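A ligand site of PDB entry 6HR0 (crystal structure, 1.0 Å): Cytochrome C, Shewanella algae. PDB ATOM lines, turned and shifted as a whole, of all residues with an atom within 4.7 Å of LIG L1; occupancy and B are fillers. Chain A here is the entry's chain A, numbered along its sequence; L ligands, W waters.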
ATOM      1  N   PHE A  32      17.353 -21.447 -27.891  1.00  0.00           N
ATOM      2  CA  PHE A  32      17.665 -21.879 -26.532  1.00  0.00           C
ATOM      3  C   PHE A  32      17.962 -20.688 -25.634  1.00  0.00           C
ATOM      4  O   PHE A  32      17.541 -20.648 -24.481  1.00  0.00           O
ATOM      5  CB  PHE A  32      18.835 -22.854 -26.595  1.00  0.00           C
ATOM      6  CG  PHE A  32      19.297 -23.424 -25.264  1.00  0.00           C
ATOM      7  CD1 PHE A  32      18.418 -23.812 -24.264  1.00  0.00           C
ATOM      8  CD2 PHE A  32      20.651 -23.674 -25.071  1.00  0.00           C
ATOM      9  CE1 PHE A  32      18.897 -24.382 -23.085  1.00  0.00           C
ATOM     10  CE2 PHE A  32      21.114 -24.250 -23.892  1.00  0.00           C
ATOM     11  CZ  PHE A  32      20.240 -24.618 -22.924  1.00  0.00           C
ATOM     12  N   GLN A  36      15.798 -19.613 -22.171  1.00  0.00           N
ATOM     13  CA  GLN A  36      16.419 -19.297 -20.900  1.00  0.00           C
ATOM     14  C   GLN A  36      16.180 -17.863 -20.491  1.00  0.00           C
ATOM     15  O   GLN A  36      16.126 -17.566 -19.289  1.00  0.00           O
ATOM     16  CB  GLN A  36      17.898 -19.601 -20.973  1.00  0.00           C
ATOM     17  CG  GLN A  36      18.183 -21.102 -21.177  1.00  0.00           C
ATOM     18  CD  GLN A  36      19.642 -21.352 -21.335  1.00  0.00           C
ATOM     19  OE1 GLN A  36      20.337 -21.712 -20.407  1.00  0.00           O
ATOM     20  NE2 GLN A  36      20.131 -21.152 -22.546  1.00  0.00           N
ATOM     21  N   HIS A  39      12.819 -18.520 -18.817  1.00  0.00           N
ATOM     22  CA  HIS A  39      12.719 -19.651 -17.915  1.00  0.00           C
ATOM     23  C   HIS A  39      13.921 -19.861 -17.020  1.00  0.00           C
ATOM     24  O   HIS A  39      13.875 -20.710 -16.130  1.00  0.00           O
ATOM     25  CB  HIS A  39      12.524 -20.949 -18.733  1.00  0.00           C
ATOM     26  CG  HIS A  39      11.190 -21.108 -19.419  1.00  0.00           C
ATOM     27  ND1 HIS A  39      10.176 -21.836 -18.833  1.00  0.00           N
ATOM     28  CD2 HIS A  39      10.717 -20.735 -20.630  1.00  0.00           C
ATOM     29  CE1 HIS A  39       9.148 -21.908 -19.665  1.00  0.00           C
ATOM     30  NE2 HIS A  39       9.456 -21.242 -20.768  1.00  0.00           N
ATOM     31  N   GLY A  40      15.029 -19.143 -17.281  1.00  0.00           N
ATOM     32  CA  GLY A  40      16.281 -19.440 -16.626  1.00  0.00           C
ATOM     33  C   GLY A  40      16.895 -20.743 -17.136  1.00  0.00           C
ATOM     34  O   GLY A  40      16.525 -21.300 -18.165  1.00  0.00           O
ATOM     35  N   SER A  41      17.879 -21.202 -16.402  1.00  0.00           N
ATOM     36  CA  SER A  41      18.735 -22.310 -16.803  1.00  0.00           C
ATOM     37  C   SER A  41      18.322 -23.649 -16.180  1.00  0.00           C
ATOM     38  O   SER A  41      17.779 -23.705 -15.070  1.00  0.00           O
ATOM     39  CB  SER A  41      20.149 -21.992 -16.341  1.00  0.00           C
ATOM     40  OG  SER A  41      20.957 -23.132 -16.438  1.00  0.00           O
ATOM     41  N   LEU A  42      18.691 -24.731 -16.879  1.00  0.00           N
ATOM     42  CA  LEU A  42      18.568 -26.085 -16.339  1.00  0.00           C
ATOM     43  C   LEU A  42      19.283 -26.237 -15.002  1.00  0.00           C
ATOM     44  O   LEU A  42      18.882 -27.052 -14.167  1.00  0.00           O
ATOM     45  CB  LEU A  42      19.193 -27.055 -17.321  1.00  0.00           C
ATOM     46  CG  LEU A  42      18.393 -27.299 -18.607  1.00  0.00           C
ATOM     47  CD1 LEU A  42      19.257 -28.040 -19.617  1.00  0.00           C
ATOM     48  CD2 LEU A  42      17.158 -28.093 -18.276  1.00  0.00           C
ATOM     49  N   MET A  45      16.899 -26.031 -12.122  1.00  0.00           N
ATOM     50  CA  MET A  45      15.669 -26.799 -12.279  1.00  0.00           C
ATOM     51  C   MET A  45      15.752 -28.124 -11.526  1.00  0.00           C
ATOM     52  O   MET A  45      16.723 -28.395 -10.793  1.00  0.00           O
ATOM     53  CB  MET A  45      15.335 -26.930 -13.750  1.00  0.00           C
ATOM     54  CG  MET A  45      15.041 -25.572 -14.371  1.00  0.00           C
ATOM     55  SD  MET A  45      14.573 -25.678 -16.083  1.00  0.00           S
ATOM     56  CE  MET A  45      12.937 -26.386 -15.964  1.00  0.00           C
ATOM     57  N   VAL A  48      14.790 -34.011 -12.968  1.00  0.00           N
ATOM     58  CA  VAL A  48      14.835 -34.485 -14.352  1.00  0.00           C
ATOM     59  C   VAL A  48      15.594 -33.519 -15.234  1.00  0.00           C
ATOM     60  O   VAL A  48      16.188 -33.934 -16.235  1.00  0.00           O
ATOM     61  CB  VAL A  48      13.473 -34.843 -14.969  1.00  0.00           C
ATOM     62  CG1 VAL A  48      12.819 -35.981 -14.204  1.00  0.00           C
ATOM     63  CG2 VAL A  48      12.562 -33.684 -15.012  1.00  0.00           C
ATOM     64  N   HIS A  49      15.580 -32.235 -14.909  1.00  0.00           N
ATOM     65  CA  HIS A  49      16.168 -31.190 -15.737  1.00  0.00           C
ATOM     66  C   HIS A  49      17.654 -30.987 -15.474  1.00  0.00           C
ATOM     67  O   HIS A  49      18.457 -31.029 -16.421  1.00  0.00           O
ATOM     68  CB  HIS A  49      15.382 -29.888 -15.487  1.00  0.00           C
ATOM     69  CG  HIS A  49      14.050 -29.854 -16.136  1.00  0.00           C
ATOM     70  ND1 HIS A  49      12.903 -30.301 -15.542  1.00  0.00           N
ATOM     71  CD2 HIS A  49      13.675 -29.446 -17.368  1.00  0.00           C
ATOM     72  CE1 HIS A  49      11.883 -30.178 -16.381  1.00  0.00           C
ATOM     73  NE2 HIS A  49      12.335 -29.678 -17.521  1.00  0.00           N
ATOM     74  N   HIS A  52      20.767 -32.624 -17.151  1.00  0.00           N
ATOM     75  CA  HIS A  52      20.948 -32.327 -18.551  1.00  0.00           C
ATOM     76  C   HIS A  52      21.606 -30.993 -18.817  1.00  0.00           C
ATOM     77  O   HIS A  52      21.822 -30.662 -19.983  1.00  0.00           O
ATOM     78  CB  HIS A  52      19.596 -32.438 -19.270  1.00  0.00           C
ATOM     79  CG  HIS A  52      19.032 -33.835 -19.217  1.00  0.00           C
ATOM     80  ND1 HIS A  52      18.113 -34.271 -18.305  1.00  0.00           N
ATOM     81  CD2 HIS A  52      19.404 -34.925 -19.927  1.00  0.00           C
ATOM     82  CE1 HIS A  52      17.894 -35.575 -18.483  1.00  0.00           C
ATOM     83  NE2 HIS A  52      18.661 -36.003 -19.478  1.00  0.00           N
ATOM     84  N   LEU A  56      21.984 -30.633 -23.185  1.00  0.00           N
ATOM     85  CA  LEU A  56      20.827 -30.477 -24.051  1.00  0.00           C
ATOM     86  C   LEU A  56      20.324 -29.052 -24.038  1.00  0.00           C
ATOM     87  O   LEU A  56      20.492 -28.316 -23.067  1.00  0.00           O
ATOM     88  CB  LEU A  56      19.644 -31.363 -23.577  1.00  0.00           C
ATOM     89  CG  LEU A  56      19.861 -32.864 -23.593  1.00  0.00           C
ATOM     90  CD1 LEU A  56      18.622 -33.530 -23.020  1.00  0.00           C
ATOM     91  CD2 LEU A  56      20.192 -33.382 -25.001  1.00  0.00           C
ATOM     92  N   MET A  57      19.652 -28.690 -25.125  1.00  0.00           N
ATOM     93  CA  MET A  57      18.821 -27.512 -25.193  1.00  0.00           C
ATOM     94  C   MET A  57      17.416 -27.893 -24.766  1.00  0.00           C
ATOM     95  O   MET A  57      16.991 -29.047 -24.907  1.00  0.00           O
ATOM     96  CB  MET A  57      18.773 -26.955 -26.612  1.00  0.00           C
ATOM     97  CG  MET A  57      20.182 -26.620 -27.169  1.00  0.00           C
ATOM     98  SD  MET A  57      20.127 -25.892 -28.776  1.00  0.00           S
ATOM     99  CE  MET A  57      19.766 -27.338 -29.741  1.00  0.00           C
ATOM    100  N   CYS A  58      16.627 -26.908 -24.304  1.00  0.00           N
ATOM    101  CA  CYS A  58      15.249 -27.218 -23.885  1.00  0.00           C
ATOM    102  C   CYS A  58      14.458 -27.930 -24.968  1.00  0.00           C
ATOM    103  O   CYS A  58      13.703 -28.875 -24.689  1.00  0.00           O
ATOM    104  CB  CYS A  58      14.491 -25.965 -23.505  1.00  0.00           C
ATOM    105  SG  CYS A  58      15.228 -24.815 -22.361  1.00  0.00           S
ATOM    106  N   CYS A  61      14.057 -31.855 -25.797  1.00  0.00           N
ATOM    107  CA  CYS A  61      12.968 -32.602 -25.157  1.00  0.00           C
ATOM    108  C   CYS A  61      11.599 -32.014 -25.448  1.00  0.00           C
ATOM    109  O   CYS A  61      10.652 -32.761 -25.728  1.00  0.00           O
ATOM    110  CB  CYS A  61      13.182 -32.668 -23.651  1.00  0.00           C
ATOM    111  SG  CYS A  61      14.671 -33.605 -23.247  1.00  0.00           S
ATOM    112  N   HIS A  62      11.455 -30.700 -25.348  1.00  0.00           N
ATOM    113  CA  HIS A  62      10.192 -29.996 -25.580  1.00  0.00           C
ATOM    114  C   HIS A  62      10.240 -29.431 -26.999  1.00  0.00           C
ATOM    115  O   HIS A  62      10.563 -28.258 -27.203  1.00  0.00           O
ATOM    116  CB  HIS A  62      10.029 -28.860 -24.576  1.00  0.00           C
ATOM    117  CG  HIS A  62      10.009 -29.250 -23.151  1.00  0.00           C
ATOM    118  ND1 HIS A  62       8.913 -29.796 -22.529  1.00  0.00           N
ATOM    119  CD2 HIS A  62      10.949 -29.093 -22.212  1.00  0.00           C
ATOM    120  CE1 HIS A  62       9.202 -29.981 -21.247  1.00  0.00           C
ATOM    121  NE2 HIS A  62      10.424 -29.541 -21.008  1.00  0.00           N
ATOM    122  N   LYS A  72       4.291 -34.488 -21.795  1.00  0.00           N
ATOM    123  CA  LYS A  72       5.500 -34.868 -21.081  1.00  0.00           C
ATOM    124  C   LYS A  72       6.497 -35.513 -22.027  1.00  0.00           C
ATOM    125  O   LYS A  72       6.183 -36.533 -22.637  1.00  0.00           O
ATOM    126  CB  LYS A  72       5.169 -35.862 -19.985  1.00  0.00           C
ATOM    127  CG  LYS A  72       4.259 -35.304 -18.906  1.00  0.00           C
ATOM    128  CD  LYS A  72       3.871 -36.410 -17.918  1.00  0.00           C
ATOM    129  CE  LYS A  72       3.171 -35.926 -16.647  1.00  0.00           C
ATOM    130  NZ  LYS A  72       1.884 -35.290 -16.983  1.00  0.00           N
ATOM    131  N   PRO A  73       7.712 -34.979 -22.138  1.00  0.00           N
ATOM    132  CA  PRO A  73       8.779 -35.692 -22.860  1.00  0.00           C
ATOM    133  C   PRO A  73       9.042 -37.024 -22.196  1.00  0.00           C
ATOM    134  O   PRO A  73       9.131 -37.098 -20.966  1.00  0.00           O
ATOM    135  CB  PRO A  73       9.975 -34.748 -22.720  1.00  0.00           C
ATOM    136  CG  PRO A  73       9.393 -33.411 -22.473  1.00  0.00           C
ATOM    137  CD  PRO A  73       8.215 -33.699 -21.578  1.00  0.00           C
ATOM    138  N   SER A  85      10.869 -41.000 -15.633  1.00  0.00           N
ATOM    139  CA  SER A  85      11.046 -39.832 -14.767  1.00  0.00           C
ATOM    140  C   SER A  85      11.308 -40.197 -13.312  1.00  0.00           C
ATOM    141  O   SER A  85      11.985 -39.448 -12.618  1.00  0.00           O
ATOM    142  CB  SER A  85       9.833 -38.921 -14.910  1.00  0.00           C
ATOM    143  OG  SER A  85       8.645 -39.564 -14.448  1.00  0.00           O
HETATM  144 FE1  LIG L   1      11.341 -29.547 -19.242  1.00  0.00          FE
HETATM  145  C1  LIG L   1       8.455 -30.394 -17.528  1.00  0.00           C
HETATM  146  C2  LIG L   1      10.503 -26.247 -19.107  1.00  0.00           C
HETATM  147  C3  LIG L   1      14.396 -28.715 -20.610  1.00  0.00           C
HETATM  148  C4  LIG L   1      11.999 -32.846 -19.772  1.00  0.00           C
HETATM  149  N1  LIG L   1       9.828 -28.526 -18.447  1.00  0.00           N
HETATM  150  C5  LIG L   1       8.723 -28.987 -17.810  1.00  0.00           C
HETATM  151  C6  LIG L   1       7.810 -28.012 -17.420  1.00  0.00           C
HETATM  152  C7  LIG L   1       8.398 -26.794 -17.908  1.00  0.00           C
HETATM  153  C8  LIG L   1       9.609 -27.181 -18.516  1.00  0.00           C
HETATM  154  C9  LIG L   1       7.849 -25.411 -17.731  1.00  0.00           C
HETATM  155  C10 LIG L   1       6.547 -28.145 -16.635  1.00  0.00           C
HETATM  156  C11 LIG L   1       5.348 -28.314 -17.497  1.00  0.00           C
HETATM  157  C12 LIG L   1       4.103 -28.362 -16.587  1.00  0.00           C
HETATM  158  O1  LIG L   1       3.711 -27.373 -15.918  1.00  0.00           O
HETATM  159  O2  LIG L   1       3.536 -29.440 -16.549  1.00  0.00           O
HETATM  160  N2  LIG L   1      12.272 -27.822 -19.733  1.00  0.00           N
HETATM  161  C13 LIG L   1      11.781 -26.574 -19.618  1.00  0.00           C
HETATM  162  C14 LIG L   1      12.675 -25.582 -20.023  1.00  0.00           C
HETATM  163  C15 LIG L   1      13.853 -26.272 -20.402  1.00  0.00           C
HETATM  164  C16 LIG L   1      13.529 -27.638 -20.235  1.00  0.00           C
HETATM  165  C17 LIG L   1      12.421 -24.107 -20.065  1.00  0.00           C
HETATM  166  C18 LIG L   1      15.192 -25.696 -20.843  1.00  0.00           C
HETATM  167  C19 LIG L   1      15.760 -24.755 -19.754  1.00  0.00           C
HETATM  168  N3  LIG L   1      12.844 -30.541 -20.080  1.00  0.00           N
HETATM  169  C20 LIG L   1      14.016 -30.070 -20.600  1.00  0.00           C
HETATM  170  C21 LIG L   1      14.835 -31.063 -21.129  1.00  0.00           C
HETATM  171  C22 LIG L   1      14.134 -32.270 -20.919  1.00  0.00           C
HETATM  172  C23 LIG L   1      12.944 -31.895 -20.257  1.00  0.00           C
HETATM  173  C24 LIG L   1      16.175 -30.856 -21.768  1.00  0.00           C
HETATM  174  C25 LIG L   1      14.506 -33.640 -21.395  1.00  0.00           C
HETATM  175  C26 LIG L   1      15.716 -34.230 -20.771  1.00  0.00           C
HETATM  176  N4  LIG L   1      10.399 -31.273 -18.773  1.00  0.00           N
HETATM  177  C27 LIG L   1      10.851 -32.522 -19.020  1.00  0.00           C
HETATM  178  C28 LIG L   1      10.026 -33.514 -18.472  1.00  0.00           C
HETATM  179  C29 LIG L   1       8.979 -32.795 -17.849  1.00  0.00           C
HETATM  180  C30 LIG L   1       9.287 -31.449 -18.043  1.00  0.00           C
HETATM  181  C31 LIG L   1      10.176 -34.986 -18.523  1.00  0.00           C
HETATM  182  C32 LIG L   1       7.814 -33.411 -17.124  1.00  0.00           C
HETATM  183  C33 LIG L   1       8.155 -33.585 -15.648  1.00  0.00           C
HETATM  184  C34 LIG L   1       6.982 -34.312 -15.006  1.00  0.00           C
HETATM  185  O3  LIG L   1       5.979 -33.642 -14.736  1.00  0.00           O
HETATM  186  O4  LIG L   1       7.051 -35.544 -14.798  1.00  0.00           O
HETATM  187 FE1  LG2 L   2      18.860 -37.888 -20.101  1.00  0.00          FE
HETATM  188  C1  LG2 L   2      22.077 -37.446 -19.116  1.00  0.00           C
HETATM  189  C2  LG2 L   2      18.025 -39.000 -16.995  1.00  0.00           C
HETATM  190  C3  LG2 L   2      15.559 -37.870 -20.969  1.00  0.00           C
HETATM  191  C4  LG2 L   2      19.744 -37.133 -23.316  1.00  0.00           C
HETATM  192  N1  LG2 L   2      19.862 -38.206 -18.409  1.00  0.00           N
HETATM  193  C5  LG2 L   2      21.152 -37.889 -18.145  1.00  0.00           C
HETATM  194  C6  LG2 L   2      21.514 -38.120 -16.812  1.00  0.00           C
HETATM  195  C7  LG2 L   2      20.323 -38.614 -16.207  1.00  0.00           C
HETATM  196  C8  LG2 L   2      19.368 -38.605 -17.214  1.00  0.00           C
HETATM  197  C9  LG2 L   2      20.160 -39.036 -14.770  1.00  0.00           C
HETATM  198  C10 LG2 L   2      22.876 -37.915 -16.226  1.00  0.00           C
HETATM  199  C11 LG2 L   2      23.832 -39.025 -16.600  1.00  0.00           C
HETATM  200  C12 LG2 L   2      23.342 -40.386 -16.218  1.00  0.00           C
HETATM  201  O1  LG2 L   2      23.376 -40.692 -14.996  1.00  0.00           O
HETATM  202  O2  LG2 L   2      22.900 -41.145 -17.099  1.00  0.00           O
HETATM  203  N2  LG2 L   2      17.127 -38.377 -19.179  1.00  0.00           N
HETATM  204  C13 LG2 L   2      16.992 -38.867 -17.920  1.00  0.00           C
HETATM  205  C14 LG2 L   2      15.639 -39.139 -17.604  1.00  0.00           C
HETATM  206  C15 LG2 L   2      14.906 -38.729 -18.758  1.00  0.00           C
HETATM  207  C16 LG2 L   2      15.874 -38.305 -19.672  1.00  0.00           C
HETATM  208  C17 LG2 L   2      15.114 -39.671 -16.309  1.00  0.00           C
HETATM  209  C18 LG2 L   2      13.430 -38.792 -18.958  1.00  0.00           C
HETATM  210  C19 LG2 L   2      12.646 -37.923 -17.972  1.00  0.00           C
HETATM  211  N3  LG2 L   2      17.861 -37.515 -21.797  1.00  0.00           N
HETATM  212  C20 LG2 L   2      16.517 -37.553 -21.980  1.00  0.00           C
HETATM  213  C21 LG2 L   2      16.133 -37.266 -23.299  1.00  0.00           C
HETATM  214  C22 LG2 L   2      17.366 -37.008 -23.976  1.00  0.00           C
HETATM  215  C23 LG2 L   2      18.369 -37.254 -23.012  1.00  0.00           C
HETATM  216  C24 LG2 L   2      14.753 -37.263 -23.847  1.00  0.00           C
HETATM  217  C25 LG2 L   2      17.556 -36.700 -25.418  1.00  0.00           C
HETATM  218  C26 LG2 L   2      16.803 -35.479 -25.917  1.00  0.00           C
HETATM  219  N4  LG2 L   2      20.594 -37.431 -21.027  1.00  0.00           N
HETATM  220  C27 LG2 L   2      20.772 -37.164 -22.332  1.00  0.00           C
HETATM  221  C28 LG2 L   2      22.093 -36.891 -22.659  1.00  0.00           C
HETATM  222  C29 LG2 L   2      22.792 -36.946 -21.437  1.00  0.00           C
HETATM  223  C30 LG2 L   2      21.796 -37.258 -20.480  1.00  0.00           C
HETATM  224  C31 LG2 L   2      22.694 -36.587 -24.012  1.00  0.00           C
HETATM  225  C32 LG2 L   2      24.266 -36.753 -21.237  1.00  0.00           C
HETATM  226  C33 LG2 L   2      24.908 -38.145 -21.328  1.00  0.00           C
HETATM  227  C34 LG2 L   2      26.424 -38.167 -21.299  1.00  0.00           C
HETATM  228  O3  LG2 L   2      27.046 -37.166 -20.910  1.00  0.00           O
HETATM  229  O4  LG2 L   2      27.004 -39.244 -21.643  1.00  0.00           O
HETATM  230 FE1  LG3 L   3       8.207 -21.157 -22.312  1.00  0.00          FE
HETATM  231  C1  LG3 L   3       5.513 -22.138 -20.402  1.00  0.00           C
HETATM  232  C2  LG3 L   3       9.079 -24.421 -22.785  1.00  0.00           C
HETATM  233  C3  LG3 L   3      10.524 -20.195 -24.631  1.00  0.00           C
HETATM  234  C4  LG3 L   3       7.725 -17.890 -21.421  1.00  0.00           C
HETATM  235  N1  LG3 L   3       7.410 -22.925 -21.761  1.00  0.00           N
HETATM  236  C5  LG3 L   3       6.320 -23.158 -21.007  1.00  0.00           C
HETATM  237  C6  LG3 L   3       6.072 -24.528 -20.821  1.00  0.00           C
HETATM  238  C7  LG3 L   3       7.135 -25.190 -21.463  1.00  0.00           C
HETATM  239  C8  LG3 L   3       7.923 -24.153 -22.022  1.00  0.00           C
HETATM  240  C9  LG3 L   3       7.390 -26.676 -21.523  1.00  0.00           C
HETATM  241  C10 LG3 L   3       4.944 -25.157 -20.082  1.00  0.00           C
HETATM  242  C11 LG3 L   3       3.667 -25.260 -20.920  1.00  0.00           C
HETATM  243  C12 LG3 L   3       2.559 -25.960 -20.110  1.00  0.00           C
HETATM  244  O1  LG3 L   3       2.573 -27.194 -20.085  1.00  0.00           O
HETATM  245  O2  LG3 L   3       1.711 -25.251 -19.550  1.00  0.00           O
HETATM  246  N2  LG3 L   3       9.546 -22.105 -23.462  1.00  0.00           N
HETATM  247  C13 LG3 L   3       9.784 -23.426 -23.515  1.00  0.00           C
HETATM  248  C14 LG3 L   3      10.821 -23.774 -24.406  1.00  0.00           C
HETATM  249  C15 LG3 L   3      11.222 -22.551 -24.962  1.00  0.00           C
HETATM  250  C16 LG3 L   3      10.426 -21.576 -24.329  1.00  0.00           C
HETATM  251  C17 LG3 L   3      11.286 -25.168 -24.751  1.00  0.00           C
HETATM  252  C18 LG3 L   3      12.280 -22.293 -26.005  1.00  0.00           C
HETATM  253  C19 LG3 L   3      12.266 -23.220 -27.210  1.00  0.00           C
HETATM  254  N3  LG3 L   3       8.975 -19.410 -22.875  1.00  0.00           N
HETATM  255  C20 LG3 L   3       9.880 -19.176 -23.886  1.00  0.00           C
HETATM  256  C21 LG3 L   3      10.136 -17.822 -24.094  1.00  0.00           C
HETATM  257  C22 LG3 L   3       9.366 -17.141 -23.108  1.00  0.00           C
HETATM  258  C23 LG3 L   3       8.682 -18.168 -22.429  1.00  0.00           C
HETATM  259  C24 LG3 L   3      11.105 -17.211 -25.086  1.00  0.00           C
HETATM  260  C25 LG3 L   3       9.334 -15.674 -22.800  1.00  0.00           C
HETATM  261  C26 LG3 L   3       9.200 -14.741 -23.973  1.00  0.00           C
HETATM  262  N4  LG3 L   3       6.889 -20.215 -21.159  1.00  0.00           N
HETATM  263  C27 LG3 L   3       6.854 -18.892 -20.871  1.00  0.00           C
HETATM  264  C28 LG3 L   3       5.886 -18.563 -19.941  1.00  0.00           C
HETATM  265  C29 LG3 L   3       5.189 -19.771 -19.664  1.00  0.00           C
HETATM  266  C30 LG3 L   3       5.885 -20.765 -20.428  1.00  0.00           C
HETATM  267  C31 LG3 L   3       5.542 -17.236 -19.385  1.00  0.00           C
HETATM  268  C32 LG3 L   3       4.002 -19.961 -18.764  1.00  0.00           C
HETATM  269  C33 LG3 L   3       2.771 -19.327 -19.477  1.00  0.00           C
HETATM  270  C34 LG3 L   3       1.439 -19.735 -18.856  1.00  0.00           C
HETATM  271  O3  LG3 L   3       1.332 -20.771 -18.176  1.00  0.00           O
HETATM  272  O4  LG3 L   3       0.453 -19.017 -19.152  1.00  0.00           O
HETATM  273  O   HOH W   1       9.971 -27.845 -14.705  1.00  0.00           O
HETATM  274  O   HOH W   2       9.395 -30.432 -14.375  1.00  0.00           O
HETATM  275  O   HOH W   3       6.826 -30.948 -13.672  1.00  0.00           O
HETATM  276  O   HOH W   4       6.950 -37.321 -16.722  1.00  0.00           O
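The backbone carbonyl oxygen (O) of Val 48 is in hydrogen-bond range of a ring nitrogen (ND1) of His 52.
His 39 touches LIG L1 (CG to C17, 3.3 Å).
Gly 40 touches LIG L1.
Leu 42 touches LIG L1 (CD2 to C3, 3.7 Å).
Met 45 touches LIG L1 (CE to C13, 3.8 Å).
CE1 of His 52 touches C26 of LIG L1, 3.4 Å away.
CD1 of Leu 56 touches C26 of LIG L1 (3.7 Å).
Met 57 touches LIG L1 (O to C24, 3.7 Å).
O of Pro 73 touches C31 of LIG L1 (3.4 Å).
Hydrophobic or aromatic side chains that line LIG L1: His 39, Leu 42, Met 45, His 49, His 52, Leu 56, His 62 and Pro 73.
Within 4 Å of LIG L1: His 39, Gly 40, Leu 42, Met 45, His 49, His 52, Leu 56, Met 57, Cys 58, Cys 61, His 62 and Pro 73.
A ring nitrogen (NE2) of His 52 is bound to an iron atom (FE1) of LG2 L2 (2.0 Å).
FE1 of LIG L1 is bound by NE2 of His 49, at 2.0 Å.
The side-chain sulfur (SG) of Cys 61 is covalently linked to a carbon (C25) of LIG L1 (1.9 Å).
The side-chain sulfur of Cys 58 is bonded to a carbon (C18) of LIG L1.
An iron atom (FE1) of LG3 L3 is bound by a ring nitrogen (NE2) of His 39.
NE2 of His 62 is bound to FE1 of LIG L1.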
